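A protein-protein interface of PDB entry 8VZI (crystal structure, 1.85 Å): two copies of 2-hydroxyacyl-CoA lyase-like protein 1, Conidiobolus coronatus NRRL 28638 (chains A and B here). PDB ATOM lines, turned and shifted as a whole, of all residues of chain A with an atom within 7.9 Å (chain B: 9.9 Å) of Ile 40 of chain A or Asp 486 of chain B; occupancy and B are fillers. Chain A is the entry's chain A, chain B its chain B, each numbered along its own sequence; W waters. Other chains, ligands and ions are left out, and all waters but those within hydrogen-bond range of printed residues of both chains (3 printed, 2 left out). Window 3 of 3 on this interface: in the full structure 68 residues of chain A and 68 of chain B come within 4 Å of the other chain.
OE2 of Glu 37 of chain A is in hydrogen-bond range of OG of Ser 490 of chain B (2.9 Å).
The backbone carbonyl oxygen of Asp 22 of chain A is in hydrogen-bond range of the backbone NH of Arg 45 of chain A (3.0 Å).
O of Arg 45 of chain A sits at hydrogen-bond distance from N of Ile 24 of chain A (2.8 Å).
Val 28 of chain A touches Ser 490 of chain B (CG1 to OG, 3.5 Å).
Val 33 of chain A touches Ser 490 of chain B.
Ala 36 of chain A touches Ser 490 of chain B.
Glu 37 of chain A touches Pro 489 of chain B.
CG2 of Ile 40 of chain A touches O of Asp 486 of chain B (3.8 Å).
Leu 488 of chain B touches Ile 40 of chain A.
Ile 40 of chain A touches Ser 490 of chain B (CD1 to N, 3.9 Å).
Arg 45 of chain A touches Ser 485 of chain B (NH2 to CB, 3.5 Å).
CD of Arg 45 of chain A touches OD1 of Asp 486 of chain B (3.4 Å).
CD2 of Phe 46 of chain A touches CB of Ser 490 of chain B, 3.5 Å away.
Of chain B, only Asp 486 (3.8 Å), Leu 488 (3.5 Å) and Ser 490 (3.9 Å) come within 4 Å of Ile 40 of chain A.
Printed residues of chain A within 4 Å of Asp 486 of chain B: Ile 40 and Arg 45.
Of chain B, only Pro 489 and Ser 490 come within 4 Å of Glu 37 of chain A.
No residue of chain B comes within 4 Å of Ala 38 of chain A.
No residue of chain B comes within 4 Å of Cys 39 of chain A.
Printed residues of chain B within 4 Å of Ala 36 of chain A: Ser 490.
Of the printed residues of chain A, Ser 490 of chain B touches Val 28 (3.5 Å), Val 33 (3.99 Å), Ala 36 (3.6 Å), Glu 37 (2.9 Å), Ile 40 (3.9 Å) and Phe 46 (3.5 Å).
Val 483 of chain B touches none of the printed residues of chain A.
The nearest residue of chain B that does not touch Ile 40 of chain A is Lys 487 of chain B (4.05 Å).
Of the 12 printed residues of chain B, 5 touch a printed residue of chain A.
Printed residues of chain A that touch a printed residue of chain B: Val 28, Val 33, Ala 36, Glu 37, Ile 40, Arg 45 and Phe 46.
Along chain A the printed residues that touch a printed residue of chain B span positions 28 to 46.
No position is printed for both chains.
Water W1 lies within hydrogen-bond range of the backbone carbonyl oxygen (O) of Ile 40 of chain A (2.6 Å), the side-chain amino group (NZ) of Lys 487 of chain B (2.7 Å) and the backbone carbonyl oxygen (O) of Asp 486 of chain B (3.0 Å).
Water W3 lies within hydrogen-bond range of O of Ser 485 of chain B (2.7 Å), O of Phe 46 of chain A (3.0 Å) and NE of Arg 45 of chain A (3.0 Å).
Water W2 lies within hydrogen-bond range of N of Val 28 of chain A (2.9 Å) and O of Ser 490 of chain B (2.9 Å).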
ATOM      1  N   ALA A  13       5.575 -19.469  41.061  1.00  0.00           N
ATOM      2  CA  ALA A  13       4.585 -19.024  40.088  1.00  0.00           C
ATOM      3  C   ALA A  13       3.171 -19.133  40.647  1.00  0.00           C
ATOM      4  O   ALA A  13       2.349 -18.228  40.458  1.00  0.00           O
ATOM      5  CB  ALA A  13       4.719 -19.830  38.798  1.00  0.00           C
ATOM      6  N   LYS A  17       0.480 -16.164  41.338  1.00  0.00           N
ATOM      7  CA  LYS A  17      -0.832 -16.248  40.701  1.00  0.00           C
ATOM      8  C   LYS A  17      -1.958 -16.110  41.723  1.00  0.00           C
ATOM      9  O   LYS A  17      -2.967 -15.440  41.454  1.00  0.00           O
ATOM     10  CB  LYS A  17      -0.955 -17.569  39.937  1.00  0.00           C
ATOM     11  CG  LYS A  17      -2.272 -17.749  39.156  1.00  0.00           C
ATOM     12  CD  LYS A  17      -2.346 -16.765  37.998  1.00  0.00           C
ATOM     13  CE  LYS A  17      -3.627 -16.925  37.159  1.00  0.00           C
ATOM     14  NZ  LYS A  17      -3.485 -16.176  35.882  1.00  0.00           N
ATOM     15  N   ASP A  22      -0.481 -10.727  37.105  1.00  0.00           N
ATOM     16  CA  ASP A  22      -0.794 -11.131  35.743  1.00  0.00           C
ATOM     17  C   ASP A  22       0.234 -10.685  34.711  1.00  0.00           C
ATOM     18  O   ASP A  22       0.104 -11.067  33.544  1.00  0.00           O
ATOM     19  CB  ASP A  22      -2.187 -10.632  35.339  1.00  0.00           C
ATOM     20  CG  ASP A  22      -2.399  -9.173  35.647  1.00  0.00           C
ATOM     21  OD1 ASP A  22      -1.431  -8.496  36.030  1.00  0.00           O
ATOM     22  OD2 ASP A  22      -3.542  -8.696  35.499  1.00  0.00           O
ATOM     23  N   VAL A  23       1.248  -9.910  35.093  1.00  0.00           N
ATOM     24  CA  VAL A  23       2.331  -9.568  34.168  1.00  0.00           C
ATOM     25  C   VAL A  23       3.610  -9.386  34.976  1.00  0.00           C
ATOM     26  O   VAL A  23       3.595  -8.834  36.082  1.00  0.00           O
ATOM     27  CB  VAL A  23       1.992  -8.320  33.304  1.00  0.00           C
ATOM     28  CG1 VAL A  23       1.831  -7.068  34.151  1.00  0.00           C
ATOM     29  CG2 VAL A  23       3.057  -8.085  32.218  1.00  0.00           C
ATOM     30  N   ILE A  24       4.713  -9.902  34.431  1.00  0.00           N
ATOM     31  CA  ILE A  24       6.044  -9.759  35.007  1.00  0.00           C
ATOM     32  C   ILE A  24       6.966  -9.188  33.943  1.00  0.00           C
ATOM     33  O   ILE A  24       6.907  -9.605  32.782  1.00  0.00           O
ATOM     34  CB  ILE A  24       6.595 -11.112  35.503  1.00  0.00           C
ATOM     35  CG1 ILE A  24       5.716 -11.674  36.625  1.00  0.00           C
ATOM     36  CG2 ILE A  24       8.060 -10.967  35.933  1.00  0.00           C
ATOM     37  CD1 ILE A  24       6.032 -13.109  36.982  1.00  0.00           C
ATOM     38  N   VAL A  28      15.607 -13.206  31.336  1.00  0.00           N
ATOM     39  CA  VAL A  28      15.924 -14.539  31.843  1.00  0.00           C
ATOM     40  C   VAL A  28      17.355 -14.988  31.568  1.00  0.00           C
ATOM     41  O   VAL A  28      18.140 -14.300  30.904  1.00  0.00           O
ATOM     42  CB  VAL A  28      14.959 -15.595  31.282  1.00  0.00           C
ATOM     43  CG1 VAL A  28      13.547 -15.297  31.734  1.00  0.00           C
ATOM     44  CG2 VAL A  28      15.063 -15.654  29.765  1.00  0.00           C
ATOM     45  N   VAL A  33      15.254 -18.971  33.952  1.00  0.00           N
ATOM     46  CA  VAL A  33      14.367 -19.237  32.813  1.00  0.00           C
ATOM     47  C   VAL A  33      13.252 -20.192  33.223  1.00  0.00           C
ATOM     48  O   VAL A  33      12.105 -20.052  32.784  1.00  0.00           O
ATOM     49  CB  VAL A  33      15.134 -19.768  31.586  1.00  0.00           C
ATOM     50  CG1 VAL A  33      15.847 -21.056  31.892  1.00  0.00           C
ATOM     51  CG2 VAL A  33      14.166 -19.978  30.415  1.00  0.00           C
ATOM     52  N   GLU A  34      13.556 -21.150  34.102  1.00  0.00           N
ATOM     53  CA  GLU A  34      12.512 -22.044  34.595  1.00  0.00           C
ATOM     54  C   GLU A  34      11.457 -21.287  35.391  1.00  0.00           C
ATOM     55  O   GLU A  34      10.276 -21.652  35.364  1.00  0.00           O
ATOM     56  CB  GLU A  34      13.120 -23.154  35.456  1.00  0.00           C
ATOM     57  CG  GLU A  34      13.862 -24.226  34.683  1.00  0.00           C
ATOM     58  CD  GLU A  34      15.363 -23.998  34.657  1.00  0.00           C
ATOM     59  OE1 GLU A  34      15.789 -22.826  34.778  1.00  0.00           O
ATOM     60  OE2 GLU A  34      16.115 -24.991  34.521  1.00  0.00           O
ATOM     61  N   VAL A  35      11.861 -20.233  36.105  1.00  0.00           N
ATOM     62  CA  VAL A  35      10.900 -19.452  36.876  1.00  0.00           C
ATOM     63  C   VAL A  35       9.960 -18.702  35.942  1.00  0.00           C
ATOM     64  O   VAL A  35       8.741 -18.688  36.143  1.00  0.00           O
ATOM     65  CB  VAL A  35      11.633 -18.493  37.832  1.00  0.00           C
ATOM     66  CG1 VAL A  35      10.653 -17.595  38.539  1.00  0.00           C
ATOM     67  CG2 VAL A  35      12.455 -19.276  38.846  1.00  0.00           C
ATOM     68  N   ALA A  36      10.517 -18.072  34.903  1.00  0.00           N
ATOM     69  CA  ALA A  36       9.680 -17.348  33.945  1.00  0.00           C
ATOM     70  C   ALA A  36       8.719 -18.284  33.222  1.00  0.00           C
ATOM     71  O   ALA A  36       7.536 -17.970  33.067  1.00  0.00           O
ATOM     72  CB  ALA A  36      10.547 -16.598  32.942  1.00  0.00           C
ATOM     73  N   GLU A  37       9.201 -19.448  32.784  1.00  0.00           N
ATOM     74  CA  GLU A  37       8.314 -20.370  32.083  1.00  0.00           C
ATOM     75  C   GLU A  37       7.235 -20.939  33.005  1.00  0.00           C
ATOM     76  O   GLU A  37       6.106 -21.188  32.557  1.00  0.00           O
ATOM     77  CB  GLU A  37       9.142 -21.474  31.430  1.00  0.00           C
ATOM     78  CG  GLU A  37      10.077 -20.934  30.312  1.00  0.00           C
ATOM     79  CD  GLU A  37       9.327 -20.282  29.119  1.00  0.00           C
ATOM     80  OE1 GLU A  37       8.319 -20.849  28.632  1.00  0.00           O
ATOM     81  OE2 GLU A  37       9.748 -19.198  28.662  1.00  0.00           O
ATOM     82  N   ALA A  38       7.542 -21.122  34.293  1.00  0.00           N
ATOM     83  CA  ALA A  38       6.511 -21.557  35.238  1.00  0.00           C
ATOM     84  C   ALA A  38       5.435 -20.489  35.422  1.00  0.00           C
ATOM     85  O   ALA A  38       4.244 -20.812  35.522  1.00  0.00           O
ATOM     86  CB  ALA A  38       7.146 -21.926  36.581  1.00  0.00           C
ATOM     87  N   CYS A  39       5.832 -19.213  35.487  1.00  0.00           N
ATOM     88  CA  CYS A  39       4.853 -18.133  35.585  1.00  0.00           C
ATOM     89  C   CYS A  39       3.971 -18.088  34.346  1.00  0.00           C
ATOM     90  O   CYS A  39       2.745 -17.954  34.448  1.00  0.00           O
ATOM     91  CB  CYS A  39       5.562 -16.791  35.790  1.00  0.00           C
ATOM     92  SG  CYS A  39       6.446 -16.660  37.375  1.00  0.00           S
ATOM     93  N   ILE A  40       4.578 -18.217  33.162  1.00  0.00           N
ATOM     94  CA  ILE A  40       3.802 -18.251  31.925  1.00  0.00           C
ATOM     95  C   ILE A  40       2.869 -19.454  31.918  1.00  0.00           C
ATOM     96  O   ILE A  40       1.725 -19.374  31.451  1.00  0.00           O
ATOM     97  CB  ILE A  40       4.749 -18.260  30.708  1.00  0.00           C
ATOM     98  CG1 ILE A  40       5.653 -17.026  30.736  1.00  0.00           C
ATOM     99  CG2 ILE A  40       3.945 -18.333  29.405  1.00  0.00           C
ATOM    100  CD1 ILE A  40       6.756 -17.025  29.667  1.00  0.00           C
ATOM    101  N   ALA A  41       3.341 -20.590  32.429  1.00  0.00           N
ATOM    102  CA  ALA A  41       2.490 -21.770  32.533  1.00  0.00           C
ATOM    103  C   ALA A  41       1.294 -21.546  33.455  1.00  0.00           C
ATOM    104  O   ALA A  41       0.278 -22.230  33.304  1.00  0.00           O
ATOM    105  CB  ALA A  41       3.312 -22.969  33.019  1.00  0.00           C
ATOM    106  N   GLU A  42       1.381 -20.604  34.391  1.00  0.00           N
ATOM    107  CA  GLU A  42       0.264 -20.299  35.279  1.00  0.00           C
ATOM    108  C   GLU A  42      -0.634 -19.190  34.744  1.00  0.00           C
ATOM    109  O   GLU A  42      -1.573 -18.782  35.440  1.00  0.00           O
ATOM    110  CB  GLU A  42       0.782 -19.922  36.679  1.00  0.00           C
ATOM    111  CG  GLU A  42       1.525 -21.054  37.378  1.00  0.00           C
ATOM    112  CD  GLU A  42       0.616 -22.220  37.743  1.00  0.00           C
ATOM    113  OE1 GLU A  42      -0.561 -21.969  38.064  1.00  0.00           O
ATOM    114  OE2 GLU A  42       1.075 -23.385  37.713  1.00  0.00           O
ATOM    115  N   GLY A  43      -0.378 -18.706  33.529  1.00  0.00           N
ATOM    116  CA  GLY A  43      -1.183 -17.655  32.939  1.00  0.00           C
ATOM    117  C   GLY A  43      -0.684 -16.253  33.188  1.00  0.00           C
ATOM    118  O   GLY A  43      -1.407 -15.291  32.898  1.00  0.00           O
ATOM    119  N   ILE A  44       0.526 -16.105  33.710  1.00  0.00           N
ATOM    120  CA  ILE A  44       1.129 -14.799  33.947  1.00  0.00           C
ATOM    121  C   ILE A  44       1.943 -14.426  32.715  1.00  0.00           C
ATOM    122  O   ILE A  44       2.830 -15.179  32.299  1.00  0.00           O
ATOM    123  CB  ILE A  44       2.011 -14.821  35.203  1.00  0.00           C
ATOM    124  CG1 ILE A  44       1.203 -15.319  36.407  1.00  0.00           C
ATOM    125  CG2 ILE A  44       2.616 -13.447  35.460  1.00  0.00           C
ATOM    126  CD1 ILE A  44       2.030 -15.381  37.701  1.00  0.00           C
ATOM    127  N   ARG A  45       1.640 -13.272  32.129  1.00  0.00           N
ATOM    128  CA  ARG A  45       2.374 -12.797  30.962  1.00  0.00           C
ATOM    129  C   ARG A  45       3.767 -12.318  31.351  1.00  0.00           C
ATOM    130  O   ARG A  45       3.955 -11.677  32.390  1.00  0.00           O
ATOM    131  CB  ARG A  45       1.603 -11.660  30.297  1.00  0.00           C
ATOM    132  CG  ARG A  45       2.241 -11.127  29.040  1.00  0.00           C
ATOM    133  CD  ARG A  45       1.314 -10.154  28.352  1.00  0.00           C
ATOM    134  NE  ARG A  45       1.912  -9.624  27.135  1.00  0.00           N
ATOM    135  CZ  ARG A  45       1.396  -8.630  26.429  1.00  0.00           C
ATOM    136  NH1 ARG A  45       0.289  -8.014  26.815  1.00  0.00           N
ATOM    137  NH2 ARG A  45       2.001  -8.253  25.306  1.00  0.00           N
ATOM    138  N   PHE A  46       4.749 -12.599  30.496  1.00  0.00           N
ATOM    139  CA  PHE A  46       6.133 -12.218  30.754  1.00  0.00           C
ATOM    140  C   PHE A  46       6.601 -11.251  29.677  1.00  0.00           C
ATOM    141  O   PHE A  46       6.528 -11.562  28.486  1.00  0.00           O
ATOM    142  CB  PHE A  46       7.053 -13.435  30.805  1.00  0.00           C
ATOM    143  CG  PHE A  46       8.434 -13.112  31.306  1.00  0.00           C
ATOM    144  CD1 PHE A  46       8.685 -13.017  32.668  1.00  0.00           C
ATOM    145  CD2 PHE A  46       9.466 -12.863  30.420  1.00  0.00           C
ATOM    146  CE1 PHE A  46       9.970 -12.699  33.143  1.00  0.00           C
ATOM    147  CE2 PHE A  46      10.747 -12.555  30.881  1.00  0.00           C
ATOM    148  CZ  PHE A  46      10.993 -12.466  32.240  1.00  0.00           C
ATOM    149  N   ILE A  47       7.079 -10.086  30.099  1.00  0.00           N
ATOM    150  CA  ILE A  47       7.590  -9.064  29.196  1.00  0.00           C
ATOM    151  C   ILE A  47       9.112  -9.113  29.303  1.00  0.00           C
ATOM    152  O   ILE A  47       9.693  -8.570  30.244  1.00  0.00           O
ATOM    153  CB  ILE A  47       7.049  -7.676  29.554  1.00  0.00           C
ATOM    154  CG1 ILE A  47       5.515  -7.693  29.584  1.00  0.00           C
ATOM    155  CG2 ILE A  47       7.578  -6.618  28.571  1.00  0.00           C
ATOM    156  CD1 ILE A  47       4.876  -7.931  28.242  1.00  0.00           C
ATOM    157  N   LEU A 430       0.598  -1.429  28.594  1.00  0.00           N
ATOM    158  CA  LEU A 430       0.031  -2.666  29.121  1.00  0.00           C
ATOM    159  C   LEU A 430      -1.160  -2.401  30.035  1.00  0.00           C
ATOM    160  O   LEU A 430      -2.071  -3.232  30.123  1.00  0.00           O
ATOM    161  CB  LEU A 430       1.116  -3.457  29.861  1.00  0.00           C
ATOM    162  CG  LEU A 430       2.135  -4.102  28.911  1.00  0.00           C
ATOM    163  CD1 LEU A 430       3.434  -4.452  29.640  1.00  0.00           C
ATOM    164  CD2 LEU A 430       1.525  -5.339  28.288  1.00  0.00           C
ATOM    165  N   ILE B 480       6.586 -15.110  15.819  1.00  0.00           N
ATOM    166  CA  ILE B 480       5.794 -14.749  16.987  1.00  0.00           C
ATOM    167  C   ILE B 480       4.466 -14.131  16.611  1.00  0.00           C
ATOM    168  O   ILE B 480       3.678 -13.793  17.507  1.00  0.00           O
ATOM    169  CB  ILE B 480       6.571 -13.811  17.934  1.00  0.00           C
ATOM    170  CG1 ILE B 480       6.842 -12.452  17.277  1.00  0.00           C
ATOM    171  CG2 ILE B 480       7.873 -14.454  18.387  1.00  0.00           C
ATOM    172  CD1 ILE B 480       7.583 -11.481  18.222  1.00  0.00           C
ATOM    173  N   SER B 482       1.820 -15.474  15.348  1.00  0.00           N
ATOM    174  CA  SER B 482       0.695 -16.342  15.676  1.00  0.00           C
ATOM    175  C   SER B 482       0.617 -16.699  17.157  1.00  0.00           C
ATOM    176  O   SER B 482      -0.327 -17.377  17.570  1.00  0.00           O
ATOM    177  CB  SER B 482       0.774 -17.628  14.846  1.00  0.00           C
ATOM    178  OG  SER B 482       2.074 -18.192  14.941  1.00  0.00           O
ATOM    179  N   VAL B 483       1.574 -16.263  17.963  1.00  0.00           N
ATOM    180  CA  VAL B 483       1.655 -16.655  19.366  1.00  0.00           C
ATOM    181  C   VAL B 483       0.814 -15.678  20.179  1.00  0.00           C
ATOM    182  O   VAL B 483       1.078 -14.468  20.128  1.00  0.00           O
ATOM    183  CB  VAL B 483       3.106 -16.665  19.857  1.00  0.00           C
ATOM    184  CG1 VAL B 483       3.175 -17.120  21.320  1.00  0.00           C
ATOM    185  CG2 VAL B 483       3.955 -17.541  18.950  1.00  0.00           C
ATOM    186  N   PRO B 484      -0.178 -16.144  20.934  1.00  0.00           N
ATOM    187  CA  PRO B 484      -0.909 -15.232  21.825  1.00  0.00           C
ATOM    188  C   PRO B 484       0.065 -14.559  22.778  1.00  0.00           C
ATOM    189  O   PRO B 484       0.960 -15.201  23.332  1.00  0.00           O
ATOM    190  CB  PRO B 484      -1.881 -16.154  22.564  1.00  0.00           C
ATOM    191  CG  PRO B 484      -1.990 -17.373  21.694  1.00  0.00           C
ATOM    192  CD  PRO B 484      -0.661 -17.532  21.034  1.00  0.00           C
ATOM    193  N   SER B 485      -0.132 -13.251  22.972  1.00  0.00           N
ATOM    194  CA  SER B 485       0.849 -12.444  23.694  1.00  0.00           C
ATOM    195  C   SER B 485       1.104 -12.980  25.101  1.00  0.00           C
ATOM    196  O   SER B 485       2.235 -12.925  25.592  1.00  0.00           O
ATOM    197  CB  SER B 485       0.390 -10.987  23.745  1.00  0.00           C
ATOM    198  OG  SER B 485       0.549 -10.356  22.484  1.00  0.00           O
ATOM    199  N   ASP B 486       0.071 -13.508  25.761  1.00  0.00           N
ATOM    200  CA  ASP B 486       0.244 -14.037  27.117  1.00  0.00           C
ATOM    201  C   ASP B 486       1.144 -15.264  27.159  1.00  0.00           C
ATOM    202  O   ASP B 486       1.716 -15.560  28.215  1.00  0.00           O
ATOM    203  CB  ASP B 486      -1.106 -14.405  27.747  1.00  0.00           C
ATOM    204  CG  ASP B 486      -1.899 -13.190  28.182  1.00  0.00           C
ATOM    205  OD1 ASP B 486      -1.424 -12.056  27.960  1.00  0.00           O
ATOM    206  OD2 ASP B 486      -2.995 -13.370  28.755  1.00  0.00           O
ATOM    207  N   LYS B 487       1.271 -15.993  26.052  1.00  0.00           N
ATOM    208  CA  LYS B 487       2.047 -17.222  26.010  1.00  0.00           C
ATOM    209  C   LYS B 487       3.394 -17.041  25.313  1.00  0.00           C
ATOM    210  O   LYS B 487       4.082 -18.029  25.044  1.00  0.00           O
ATOM    211  CB  LYS B 487       1.230 -18.328  25.332  1.00  0.00           C
ATOM    212  CG  LYS B 487      -0.079 -18.716  26.087  1.00  0.00           C
ATOM    213  CD  LYS B 487       0.251 -19.438  27.398  1.00  0.00           C
ATOM    214  CE  LYS B 487      -0.988 -19.829  28.215  1.00  0.00           C
ATOM    215  NZ  LYS B 487      -1.594 -18.695  28.992  1.00  0.00           N
ATOM    216  N   LEU B 488       3.792 -15.809  25.027  1.00  0.00           N
ATOM    217  CA  LEU B 488       5.062 -15.590  24.363  1.00  0.00           C
ATOM    218  C   LEU B 488       6.188 -16.051  25.285  1.00  0.00           C
ATOM    219  O   LEU B 488       6.199 -15.689  26.469  1.00  0.00           O
ATOM    220  CB  LEU B 488       5.236 -14.120  23.997  1.00  0.00           C
ATOM    221  CG  LEU B 488       6.528 -13.731  23.276  1.00  0.00           C
ATOM    222  CD1 LEU B 488       6.489 -14.178  21.824  1.00  0.00           C
ATOM    223  CD2 LEU B 488       6.765 -12.222  23.381  1.00  0.00           C
ATOM    224  N   PRO B 489       7.114 -16.878  24.801  1.00  0.00           N
ATOM    225  CA  PRO B 489       8.143 -17.440  25.685  1.00  0.00           C
ATOM    226  C   PRO B 489       9.182 -16.405  26.078  1.00  0.00           C
ATOM    227  O   PRO B 489       9.488 -15.473  25.329  1.00  0.00           O
ATOM    228  CB  PRO B 489       8.768 -18.561  24.847  1.00  0.00           C
ATOM    229  CG  PRO B 489       7.782 -18.827  23.739  1.00  0.00           C
ATOM    230  CD  PRO B 489       7.093 -17.522  23.476  1.00  0.00           C
ATOM    231  N   SER B 490       9.752 -16.601  27.272  1.00  0.00           N
ATOM    232  CA  SER B 490      10.608 -15.590  27.875  1.00  0.00           C
ATOM    233  C   SER B 490      11.964 -15.485  27.194  1.00  0.00           C
ATOM    234  O   SER B 490      12.630 -14.450  27.317  1.00  0.00           O
ATOM    235  CB  SER B 490      10.810 -15.908  29.359  1.00  0.00           C
ATOM    236  OG  SER B 490      11.541 -17.122  29.501  1.00  0.00           O
ATOM    237  N   PHE B 491      12.394 -16.525  26.494  1.00  0.00           N
ATOM    238  CA  PHE B 491      13.708 -16.523  25.868  1.00  0.00           C
ATOM    239  C   PHE B 491      13.718 -15.881  24.490  1.00  0.00           C
ATOM    240  O   PHE B 491      14.800 -15.598  23.971  1.00  0.00           O
ATOM    241  CB  PHE B 491      14.241 -17.953  25.744  1.00  0.00           C
ATOM    242  CG  PHE B 491      13.319 -18.874  25.002  1.00  0.00           C
ATOM    243  CD1 PHE B 491      13.306 -18.897  23.614  1.00  0.00           C
ATOM    244  CD2 PHE B 491      12.453 -19.710  25.691  1.00  0.00           C
ATOM    245  CE1 PHE B 491      12.456 -19.730  22.925  1.00  0.00           C
ATOM    246  CE2 PHE B 491      11.603 -20.556  25.002  1.00  0.00           C
ATOM    247  CZ  PHE B 491      11.602 -20.563  23.621  1.00  0.00           C
ATOM    248  N   THR B 492      12.567 -15.647  23.872  1.00  0.00           N
ATOM    249  CA  THR B 492      12.626 -15.205  22.481  1.00  0.00           C
ATOM    250  C   THR B 492      12.663 -13.686  22.385  1.00  0.00           C
ATOM    251  O   THR B 492      12.128 -12.960  23.231  1.00  0.00           O
ATOM    252  CB  THR B 492      11.458 -15.745  21.650  1.00  0.00           C
ATOM    253  OG1 THR B 492      11.749 -15.553  20.253  1.00  0.00           O
ATOM    254  CG2 THR B 492      10.140 -15.025  21.989  1.00  0.00           C
HETATM  255  O   HOH W   1       0.455 -17.436  30.175  1.00  0.00           O
HETATM  256  O   HOH W   2      14.079 -12.527  28.967  1.00  0.00           O
HETATM  257  O   HOH W   3       4.249 -11.391  26.582  1.00  0.00           O
